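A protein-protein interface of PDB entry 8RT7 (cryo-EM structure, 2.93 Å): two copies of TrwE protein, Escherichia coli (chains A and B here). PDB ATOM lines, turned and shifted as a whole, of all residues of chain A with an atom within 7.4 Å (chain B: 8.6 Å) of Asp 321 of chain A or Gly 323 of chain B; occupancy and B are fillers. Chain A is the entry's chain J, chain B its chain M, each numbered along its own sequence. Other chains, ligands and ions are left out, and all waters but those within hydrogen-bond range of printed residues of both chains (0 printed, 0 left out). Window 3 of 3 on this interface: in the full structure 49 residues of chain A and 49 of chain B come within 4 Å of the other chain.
The backbone carbonyl oxygen of Asp 324 of chain B sits at hydrogen-bond distance from the side-chain hydroxyl of Ser 327 of chain B.
O of Gly 323 of chain B sits at hydrogen-bond distance from OG of Ser 327 of chain B, at 3.3 Å.
The backbone carbonyl oxygen (O) of Asp 324 of chain A sits at hydrogen-bond distance from the side-chain hydroxyl (OG) of Ser 327 of chain A (3.0 Å).
CG1 of Ile 314 of chain A touches CD1 of Ile 319 of chain B, 3.9 Å away.
OD2 of Asp 321 of chain A touches CA of Gly 323 of chain B, 3.2 Å away.
CB of Ser 327 of chain B touches O of Asp 321 of chain A (3.7 Å).
OG of Ser 327 of chain B touches OD2 of Asp 324 of chain A, 3.8 Å away.
Trp 325 of chain A touches Ala 326 of chain B.
Trp 325 of chain A touches Gly 330 of chain B.
Printed residues of chain B within 4 Å of Asp 321 of chain A: Gly 323 (3.2 Å) and Ser 327 (3.7 Å).
Of chain A, only Asp 321 comes within 4 Å of Gly 323 of chain B.
Gly 320 of chain A touches none of the printed residues of chain B.
Of the printed residues of chain B, Trp 325 of chain A touches Ala 326 (3.996 Å) and Gly 330 (3.3 Å).
Of the printed residues of chain B, Ile 314 of chain A touches Ile 319 (3.9 Å).
Of the printed residues of chain A, Ser 327 of chain B touches Asp 321 (3.7 Å) and Asp 324 (3.8 Å).
Ser 317 of chain A touches none of the printed residues of chain B.
Ile 316 of chain A touches none of the printed residues of chain B.
The nearest printed residue of chain B that does not touch Asp 321 of chain A is Asp 324 of chain B (4.02 Å).
The nearest residue of chain A that does not touch Gly 323 of chain B is Leu 318 of chain A (4.9 Å).
Among the printed residues, no Asp or Glu carboxylate lies within 4 Å of a Lys or Arg side-chain nitrogen of the other chain.
Asp 321 of chain A touches Gly 323 of chain B, but with the chains exchanged Gly 323 of chain A does not touch Asp 321 of chain B (13.5 Å).
Asp 321 of chain A touches Ser 327 of chain B, but with the chains exchanged Ser 327 of chain A does not touch Asp 321 of chain B (16.2 Å).
Asp 324 of chain A touches Ser 327 of chain B, but with the chains exchanged Ser 327 of chain A does not touch Asp 324 of chain B (12.0 Å).
Trp 325 of chain A touches Ala 326 of chain B, but with the chains exchanged Ala 326 of chain A does not touch Trp 325 of chain B (11.1 Å).
Of the 6 pairs that touch across the chains among the printed residues, none has its exchanged pair printed and touching as well.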
ATOM      1  N   ILE A 314      -4.231 -11.684 -14.622  1.00  0.00           N
ATOM      2  CA  ILE A 314      -3.022 -12.158 -13.961  1.00  0.00           C
ATOM      3  C   ILE A 314      -3.368 -12.932 -12.700  1.00  0.00           C
ATOM      4  O   ILE A 314      -2.797 -13.995 -12.432  1.00  0.00           O
ATOM      5  CB  ILE A 314      -2.084 -10.979 -13.661  1.00  0.00           C
ATOM      6  CG1 ILE A 314      -1.420 -10.492 -14.944  1.00  0.00           C
ATOM      7  CG2 ILE A 314      -1.049 -11.367 -12.630  1.00  0.00           C
ATOM      8  CD1 ILE A 314      -0.854  -9.116 -14.821  1.00  0.00           C
ATOM      9  N   MET A 315      -4.305 -12.420 -11.907  1.00  0.00           N
ATOM     10  CA  MET A 315      -4.697 -13.101 -10.684  1.00  0.00           C
ATOM     11  C   MET A 315      -5.406 -14.409 -10.983  1.00  0.00           C
ATOM     12  O   MET A 315      -5.202 -15.398 -10.280  1.00  0.00           O
ATOM     13  CB  MET A 315      -5.583 -12.189  -9.846  1.00  0.00           C
ATOM     14  CG  MET A 315      -6.115 -12.836  -8.606  1.00  0.00           C
ATOM     15  SD  MET A 315      -7.782 -12.285  -8.254  1.00  0.00           S
ATOM     16  CE  MET A 315      -8.629 -12.790  -9.741  1.00  0.00           C
ATOM     17  N   ILE A 316      -6.237 -14.443 -12.024  1.00  0.00           N
ATOM     18  CA  ILE A 316      -6.889 -15.688 -12.406  1.00  0.00           C
ATOM     19  C   ILE A 316      -5.856 -16.724 -12.825  1.00  0.00           C
ATOM     20  O   ILE A 316      -5.932 -17.892 -12.427  1.00  0.00           O
ATOM     21  CB  ILE A 316      -7.918 -15.425 -13.518  1.00  0.00           C
ATOM     22  CG1 ILE A 316      -9.189 -14.826 -12.928  1.00  0.00           C
ATOM     23  CG2 ILE A 316      -8.228 -16.686 -14.263  1.00  0.00           C
ATOM     24  CD1 ILE A 316      -9.878 -15.728 -11.947  1.00  0.00           C
ATOM     25  N   SER A 317      -4.869 -16.314 -13.622  1.00  0.00           N
ATOM     26  CA  SER A 317      -3.835 -17.250 -14.047  1.00  0.00           C
ATOM     27  C   SER A 317      -3.028 -17.764 -12.865  1.00  0.00           C
ATOM     28  O   SER A 317      -2.747 -18.964 -12.772  1.00  0.00           O
ATOM     29  CB  SER A 317      -2.917 -16.585 -15.064  1.00  0.00           C
ATOM     30  OG  SER A 317      -1.891 -17.473 -15.457  1.00  0.00           O
ATOM     31  N   LEU A 318      -2.644 -16.878 -11.949  1.00  0.00           N
ATOM     32  CA  LEU A 318      -1.847 -17.314 -10.810  1.00  0.00           C
ATOM     33  C   LEU A 318      -2.654 -18.190  -9.865  1.00  0.00           C
ATOM     34  O   LEU A 318      -2.118 -19.136  -9.282  1.00  0.00           O
ATOM     35  CB  LEU A 318      -1.272 -16.112 -10.071  1.00  0.00           C
ATOM     36  CG  LEU A 318      -0.190 -15.340 -10.817  1.00  0.00           C
ATOM     37  CD1 LEU A 318       0.669 -14.582  -9.834  1.00  0.00           C
ATOM     38  CD2 LEU A 318       0.654 -16.282 -11.642  1.00  0.00           C
ATOM     39  N   ILE A 319      -3.944 -17.898  -9.700  1.00  0.00           N
ATOM     40  CA  ILE A 319      -4.796 -18.742  -8.870  1.00  0.00           C
ATOM     41  C   ILE A 319      -4.925 -20.126  -9.481  1.00  0.00           C
ATOM     42  O   ILE A 319      -4.816 -21.139  -8.783  1.00  0.00           O
ATOM     43  CB  ILE A 319      -6.169 -18.076  -8.667  1.00  0.00           C
ATOM     44  CG1 ILE A 319      -6.072 -16.987  -7.603  1.00  0.00           C
ATOM     45  CG2 ILE A 319      -7.215 -19.101  -8.287  1.00  0.00           C
ATOM     46  CD1 ILE A 319      -5.604 -17.493  -6.278  1.00  0.00           C
ATOM     47  N   GLY A 320      -5.143 -20.197 -10.793  1.00  0.00           N
ATOM     48  CA  GLY A 320      -5.211 -21.492 -11.444  1.00  0.00           C
ATOM     49  C   GLY A 320      -3.923 -22.279 -11.301  1.00  0.00           C
ATOM     50  O   GLY A 320      -3.939 -23.471 -10.986  1.00  0.00           O
ATOM     51  N   ASP A 321      -2.785 -21.618 -11.518  1.00  0.00           N
ATOM     52  CA  ASP A 321      -1.506 -22.318 -11.439  1.00  0.00           C
ATOM     53  C   ASP A 321      -1.202 -22.776 -10.017  1.00  0.00           C
ATOM     54  O   ASP A 321      -0.731 -23.900  -9.810  1.00  0.00           O
ATOM     55  CB  ASP A 321      -0.393 -21.426 -11.981  1.00  0.00           C
ATOM     56  CG  ASP A 321      -0.520 -21.185 -13.478  1.00  0.00           C
ATOM     57  OD1 ASP A 321      -1.259 -21.943 -14.142  1.00  0.00           O
ATOM     58  OD2 ASP A 321       0.116 -20.243 -13.995  1.00  0.00           O
ATOM     59  N   LEU A 322      -1.477 -21.933  -9.021  1.00  0.00           N
ATOM     60  CA  LEU A 322      -1.258 -22.328  -7.634  1.00  0.00           C
ATOM     61  C   LEU A 322      -2.186 -23.464  -7.220  1.00  0.00           C
ATOM     62  O   LEU A 322      -1.765 -24.385  -6.511  1.00  0.00           O
ATOM     63  CB  LEU A 322      -1.435 -21.119  -6.720  1.00  0.00           C
ATOM     64  CG  LEU A 322      -1.090 -21.245  -5.239  1.00  0.00           C
ATOM     65  CD1 LEU A 322      -0.700 -19.887  -4.697  1.00  0.00           C
ATOM     66  CD2 LEU A 322      -2.285 -21.768  -4.467  1.00  0.00           C
ATOM     67  N   GLY A 323      -3.453 -23.409  -7.626  1.00  0.00           N
ATOM     68  CA  GLY A 323      -4.356 -24.497  -7.303  1.00  0.00           C
ATOM     69  C   GLY A 323      -3.942 -25.794  -7.960  1.00  0.00           C
ATOM     70  O   GLY A 323      -4.063 -26.868  -7.369  1.00  0.00           O
ATOM     71  N   ASP A 324      -3.449 -25.713  -9.195  1.00  0.00           N
ATOM     72  CA  ASP A 324      -2.913 -26.893  -9.857  1.00  0.00           C
ATOM     73  C   ASP A 324      -1.729 -27.461  -9.088  1.00  0.00           C
ATOM     74  O   ASP A 324      -1.624 -28.678  -8.902  1.00  0.00           O
ATOM     75  CB  ASP A 324      -2.509 -26.542 -11.284  1.00  0.00           C
ATOM     76  CG  ASP A 324      -1.762 -27.656 -11.963  1.00  0.00           C
ATOM     77  OD1 ASP A 324      -2.193 -28.820 -11.841  1.00  0.00           O
ATOM     78  OD2 ASP A 324      -0.739 -27.368 -12.618  1.00  0.00           O
ATOM     79  N   TRP A 325      -0.836 -26.591  -8.620  1.00  0.00           N
ATOM     80  CA  TRP A 325       0.292 -27.048  -7.816  1.00  0.00           C
ATOM     81  C   TRP A 325      -0.185 -27.764  -6.561  1.00  0.00           C
ATOM     82  O   TRP A 325       0.284 -28.863  -6.238  1.00  0.00           O
ATOM     83  CB  TRP A 325       1.174 -25.861  -7.448  1.00  0.00           C
ATOM     84  CG  TRP A 325       2.149 -26.139  -6.357  1.00  0.00           C
ATOM     85  CD1 TRP A 325       3.395 -26.662  -6.497  1.00  0.00           C
ATOM     86  CD2 TRP A 325       1.973 -25.889  -4.959  1.00  0.00           C
ATOM     87  NE1 TRP A 325       4.007 -26.761  -5.275  1.00  0.00           N
ATOM     88  CE2 TRP A 325       3.154 -26.292  -4.313  1.00  0.00           C
ATOM     89  CE3 TRP A 325       0.932 -25.365  -4.192  1.00  0.00           C
ATOM     90  CZ2 TRP A 325       3.324 -26.190  -2.936  1.00  0.00           C
ATOM     91  CZ3 TRP A 325       1.100 -25.267  -2.824  1.00  0.00           C
ATOM     92  CH2 TRP A 325       2.287 -25.676  -2.210  1.00  0.00           C
ATOM     93  N   ALA A 326      -1.130 -27.156  -5.845  1.00  0.00           N
ATOM     94  CA  ALA A 326      -1.592 -27.730  -4.587  1.00  0.00           C
ATOM     95  C   ALA A 326      -2.316 -29.052  -4.807  1.00  0.00           C
ATOM     96  O   ALA A 326      -2.194 -29.972  -3.992  1.00  0.00           O
ATOM     97  CB  ALA A 326      -2.490 -26.737  -3.857  1.00  0.00           C
ATOM     98  N   SER A 327      -3.077 -29.171  -5.899  1.00  0.00           N
ATOM     99  CA  SER A 327      -3.732 -30.442  -6.185  1.00  0.00           C
ATOM    100  C   SER A 327      -2.715 -31.502  -6.584  1.00  0.00           C
ATOM    101  O   SER A 327      -2.893 -32.685  -6.277  1.00  0.00           O
ATOM    102  CB  SER A 327      -4.784 -30.274  -7.281  1.00  0.00           C
ATOM    103  OG  SER A 327      -4.185 -30.130  -8.553  1.00  0.00           O
ATOM    104  N   ILE B 316       1.925 -11.208 -20.425  1.00  0.00           N
ATOM    105  CA  ILE B 316       1.015 -12.326 -20.208  1.00  0.00           C
ATOM    106  C   ILE B 316       1.730 -13.643 -20.461  1.00  0.00           C
ATOM    107  O   ILE B 316       1.634 -14.580 -19.663  1.00  0.00           O
ATOM    108  CB  ILE B 316      -0.234 -12.183 -21.097  1.00  0.00           C
ATOM    109  CG1 ILE B 316      -1.209 -11.174 -20.498  1.00  0.00           C
ATOM    110  CG2 ILE B 316      -0.922 -13.509 -21.264  1.00  0.00           C
ATOM    111  CD1 ILE B 316      -1.715 -11.548 -19.136  1.00  0.00           C
ATOM    112  N   SER B 317       2.471 -13.733 -21.568  1.00  0.00           N
ATOM    113  CA  SER B 317       3.170 -14.976 -21.876  1.00  0.00           C
ATOM    114  C   SER B 317       4.237 -15.293 -20.839  1.00  0.00           C
ATOM    115  O   SER B 317       4.378 -16.446 -20.420  1.00  0.00           O
ATOM    116  CB  SER B 317       3.788 -14.901 -23.266  1.00  0.00           C
ATOM    117  OG  SER B 317       2.795 -15.047 -24.261  1.00  0.00           O
ATOM    118  N   LEU B 318       4.999 -14.287 -20.411  1.00  0.00           N
ATOM    119  CA  LEU B 318       6.038 -14.533 -19.417  1.00  0.00           C
ATOM    120  C   LEU B 318       5.444 -14.947 -18.079  1.00  0.00           C
ATOM    121  O   LEU B 318       5.984 -15.828 -17.404  1.00  0.00           O
ATOM    122  CB  LEU B 318       6.915 -13.298 -19.252  1.00  0.00           C
ATOM    123  CG  LEU B 318       7.830 -12.983 -20.431  1.00  0.00           C
ATOM    124  CD1 LEU B 318       8.675 -11.765 -20.117  1.00  0.00           C
ATOM    125  CD2 LEU B 318       8.697 -14.179 -20.785  1.00  0.00           C
ATOM    126  N   ILE B 319       4.336 -14.326 -17.676  1.00  0.00           N
ATOM    127  CA  ILE B 319       3.696 -14.692 -16.418  1.00  0.00           C
ATOM    128  C   ILE B 319       3.115 -16.097 -16.502  1.00  0.00           C
ATOM    129  O   ILE B 319       3.187 -16.867 -15.541  1.00  0.00           O
ATOM    130  CB  ILE B 319       2.633 -13.646 -16.040  1.00  0.00           C
ATOM    131  CG1 ILE B 319       3.296 -12.444 -15.371  1.00  0.00           C
ATOM    132  CG2 ILE B 319       1.573 -14.242 -15.146  1.00  0.00           C
ATOM    133  CD1 ILE B 319       2.340 -11.360 -14.987  1.00  0.00           C
ATOM    134  N   GLY B 320       2.547 -16.462 -17.651  1.00  0.00           N
ATOM    135  CA  GLY B 320       2.063 -17.821 -17.818  1.00  0.00           C
ATOM    136  C   GLY B 320       3.176 -18.847 -17.750  1.00  0.00           C
ATOM    137  O   GLY B 320       3.026 -19.904 -17.133  1.00  0.00           O
ATOM    138  N   ASP B 321       4.315 -18.546 -18.373  1.00  0.00           N
ATOM    139  CA  ASP B 321       5.448 -19.464 -18.310  1.00  0.00           C
ATOM    140  C   ASP B 321       5.991 -19.572 -16.892  1.00  0.00           C
ATOM    141  O   ASP B 321       6.355 -20.664 -16.446  1.00  0.00           O
ATOM    142  CB  ASP B 321       6.542 -19.016 -19.276  1.00  0.00           C
ATOM    143  CG  ASP B 321       6.186 -19.291 -20.727  1.00  0.00           C
ATOM    144  OD1 ASP B 321       5.555 -20.333 -20.997  1.00  0.00           O
ATOM    145  OD2 ASP B 321       6.534 -18.464 -21.597  1.00  0.00           O
ATOM    146  N   LEU B 322       6.065 -18.454 -16.170  1.00  0.00           N
ATOM    147  CA  LEU B 322       6.524 -18.496 -14.785  1.00  0.00           C
ATOM    148  C   LEU B 322       5.563 -19.299 -13.915  1.00  0.00           C
ATOM    149  O   LEU B 322       5.991 -20.048 -13.029  1.00  0.00           O
ATOM    150  CB  LEU B 322       6.694 -17.072 -14.257  1.00  0.00           C
ATOM    151  CG  LEU B 322       7.194 -16.768 -12.842  1.00  0.00           C
ATOM    152  CD1 LEU B 322       7.667 -15.330 -12.791  1.00  0.00           C
ATOM    153  CD2 LEU B 322       6.121 -16.977 -11.785  1.00  0.00           C
ATOM    154  N   GLY B 323       4.262 -19.149 -14.146  1.00  0.00           N
ATOM    155  CA  GLY B 323       3.300 -19.962 -13.427  1.00  0.00           C
ATOM    156  C   GLY B 323       3.468 -21.440 -13.713  1.00  0.00           C
ATOM    157  O   GLY B 323       3.401 -22.267 -12.803  1.00  0.00           O
ATOM    158  N   ASP B 324       3.687 -21.793 -14.980  1.00  0.00           N
ATOM    159  CA  ASP B 324       3.926 -23.191 -15.318  1.00  0.00           C
ATOM    160  C   ASP B 324       5.192 -23.717 -14.656  1.00  0.00           C
ATOM    161  O   ASP B 324       5.222 -24.855 -14.183  1.00  0.00           O
ATOM    162  CB  ASP B 324       4.011 -23.370 -16.831  1.00  0.00           C
ATOM    163  CG  ASP B 324       2.661 -23.593 -17.463  1.00  0.00           C
ATOM    164  OD1 ASP B 324       2.599 -23.713 -18.703  1.00  0.00           O
ATOM    165  OD2 ASP B 324       1.660 -23.651 -16.720  1.00  0.00           O
ATOM    166  N   TRP B 325       6.248 -22.908 -14.621  1.00  0.00           N
ATOM    167  CA  TRP B 325       7.492 -23.347 -13.996  1.00  0.00           C
ATOM    168  C   TRP B 325       7.314 -23.560 -12.501  1.00  0.00           C
ATOM    169  O   TRP B 325       7.801 -24.554 -11.946  1.00  0.00           O
ATOM    170  CB  TRP B 325       8.589 -22.327 -14.268  1.00  0.00           C
ATOM    171  CG  TRP B 325       9.825 -22.517 -13.462  1.00  0.00           C
ATOM    172  CD1 TRP B 325      10.874 -23.334 -13.752  1.00  0.00           C
ATOM    173  CD2 TRP B 325      10.161 -21.850 -12.244  1.00  0.00           C
ATOM    174  NE1 TRP B 325      11.839 -23.225 -12.785  1.00  0.00           N
ATOM    175  CE2 TRP B 325      11.424 -22.318 -11.847  1.00  0.00           C
ATOM    176  CE3 TRP B 325       9.512 -20.904 -11.449  1.00  0.00           C
ATOM    177  CZ2 TRP B 325      12.051 -21.876 -10.691  1.00  0.00           C
ATOM    178  CZ3 TRP B 325      10.136 -20.466 -10.303  1.00  0.00           C
ATOM    179  CH2 TRP B 325      11.395 -20.950  -9.934  1.00  0.00           C
ATOM    180  N   ALA B 326       6.606 -22.649 -11.834  1.00  0.00           N
ATOM    181  CA  ALA B 326       6.354 -22.814 -10.407  1.00  0.00           C
ATOM    182  C   ALA B 326       5.466 -24.021 -10.134  1.00  0.00           C
ATOM    183  O   ALA B 326       5.678 -24.739  -9.153  1.00  0.00           O
ATOM    184  CB  ALA B 326       5.732 -21.546  -9.832  1.00  0.00           C
ATOM    185  N   SER B 327       4.463 -24.261 -10.981  1.00  0.00           N
ATOM    186  CA  SER B 327       3.566 -25.387 -10.743  1.00  0.00           C
ATOM    187  C   SER B 327       4.231 -26.715 -11.090  1.00  0.00           C
ATOM    188  O   SER B 327       3.858 -27.760 -10.547  1.00  0.00           O
ATOM    189  CB  SER B 327       2.271 -25.211 -11.534  1.00  0.00           C
ATOM    190  OG  SER B 327       2.485 -25.406 -12.918  1.00  0.00           O
ATOM    191  N   ARG B 328       5.199 -26.703 -12.007  1.00  0.00           N
ATOM    192  CA  ARG B 328       5.969 -27.912 -12.274  1.00  0.00           C
ATOM    193  C   ARG B 328       7.038 -28.136 -11.217  1.00  0.00           C
ATOM    194  O   ARG B 328       7.524 -29.261 -11.059  1.00  0.00           O
ATOM    195  CB  ARG B 328       6.606 -27.850 -13.661  1.00  0.00           C
ATOM    196  CG  ARG B 328       5.627 -28.069 -14.803  1.00  0.00           C
ATOM    197  CD  ARG B 328       5.015 -29.454 -14.738  1.00  0.00           C
ATOM    198  NE  ARG B 328       4.251 -29.766 -15.942  1.00  0.00           N
ATOM    199  CZ  ARG B 328       4.775 -30.283 -17.048  1.00  0.00           C
ATOM    200  NH1 ARG B 328       6.073 -30.547 -17.109  1.00  0.00           N
ATOM    201  NH2 ARG B 328       4.003 -30.534 -18.095  1.00  0.00           N
ATOM    202  N   GLN B 329       7.409 -27.090 -10.480  1.00  0.00           N
ATOM    203  CA  GLN B 329       8.362 -27.244  -9.391  1.00  0.00           C
ATOM    204  C   GLN B 329       7.713 -27.742  -8.109  1.00  0.00           C
ATOM    205  O   GLN B 329       8.281 -27.565  -7.026  1.00  0.00           O
ATOM    206  CB  GLN B 329       9.090 -25.925  -9.132  1.00  0.00           C
ATOM    207  CG  GLN B 329      10.528 -26.107  -8.692  1.00  0.00           C
ATOM    208  CD  GLN B 329      11.195 -24.802  -8.336  1.00  0.00           C
ATOM    209  OE1 GLN B 329      10.610 -23.732  -8.495  1.00  0.00           O
ATOM    210  NE2 GLN B 329      12.424 -24.881  -7.843  1.00  0.00           N
ATOM    211  N   GLY B 330       6.527 -28.345  -8.208  1.00  0.00           N
ATOM    212  CA  GLY B 330       5.877 -28.878  -7.023  1.00  0.00           C
ATOM    213  C   GLY B 330       6.667 -29.999  -6.376  1.00  0.00           C
ATOM    214  O   GLY B 330       6.680 -30.135  -5.150  1.00  0.00           O
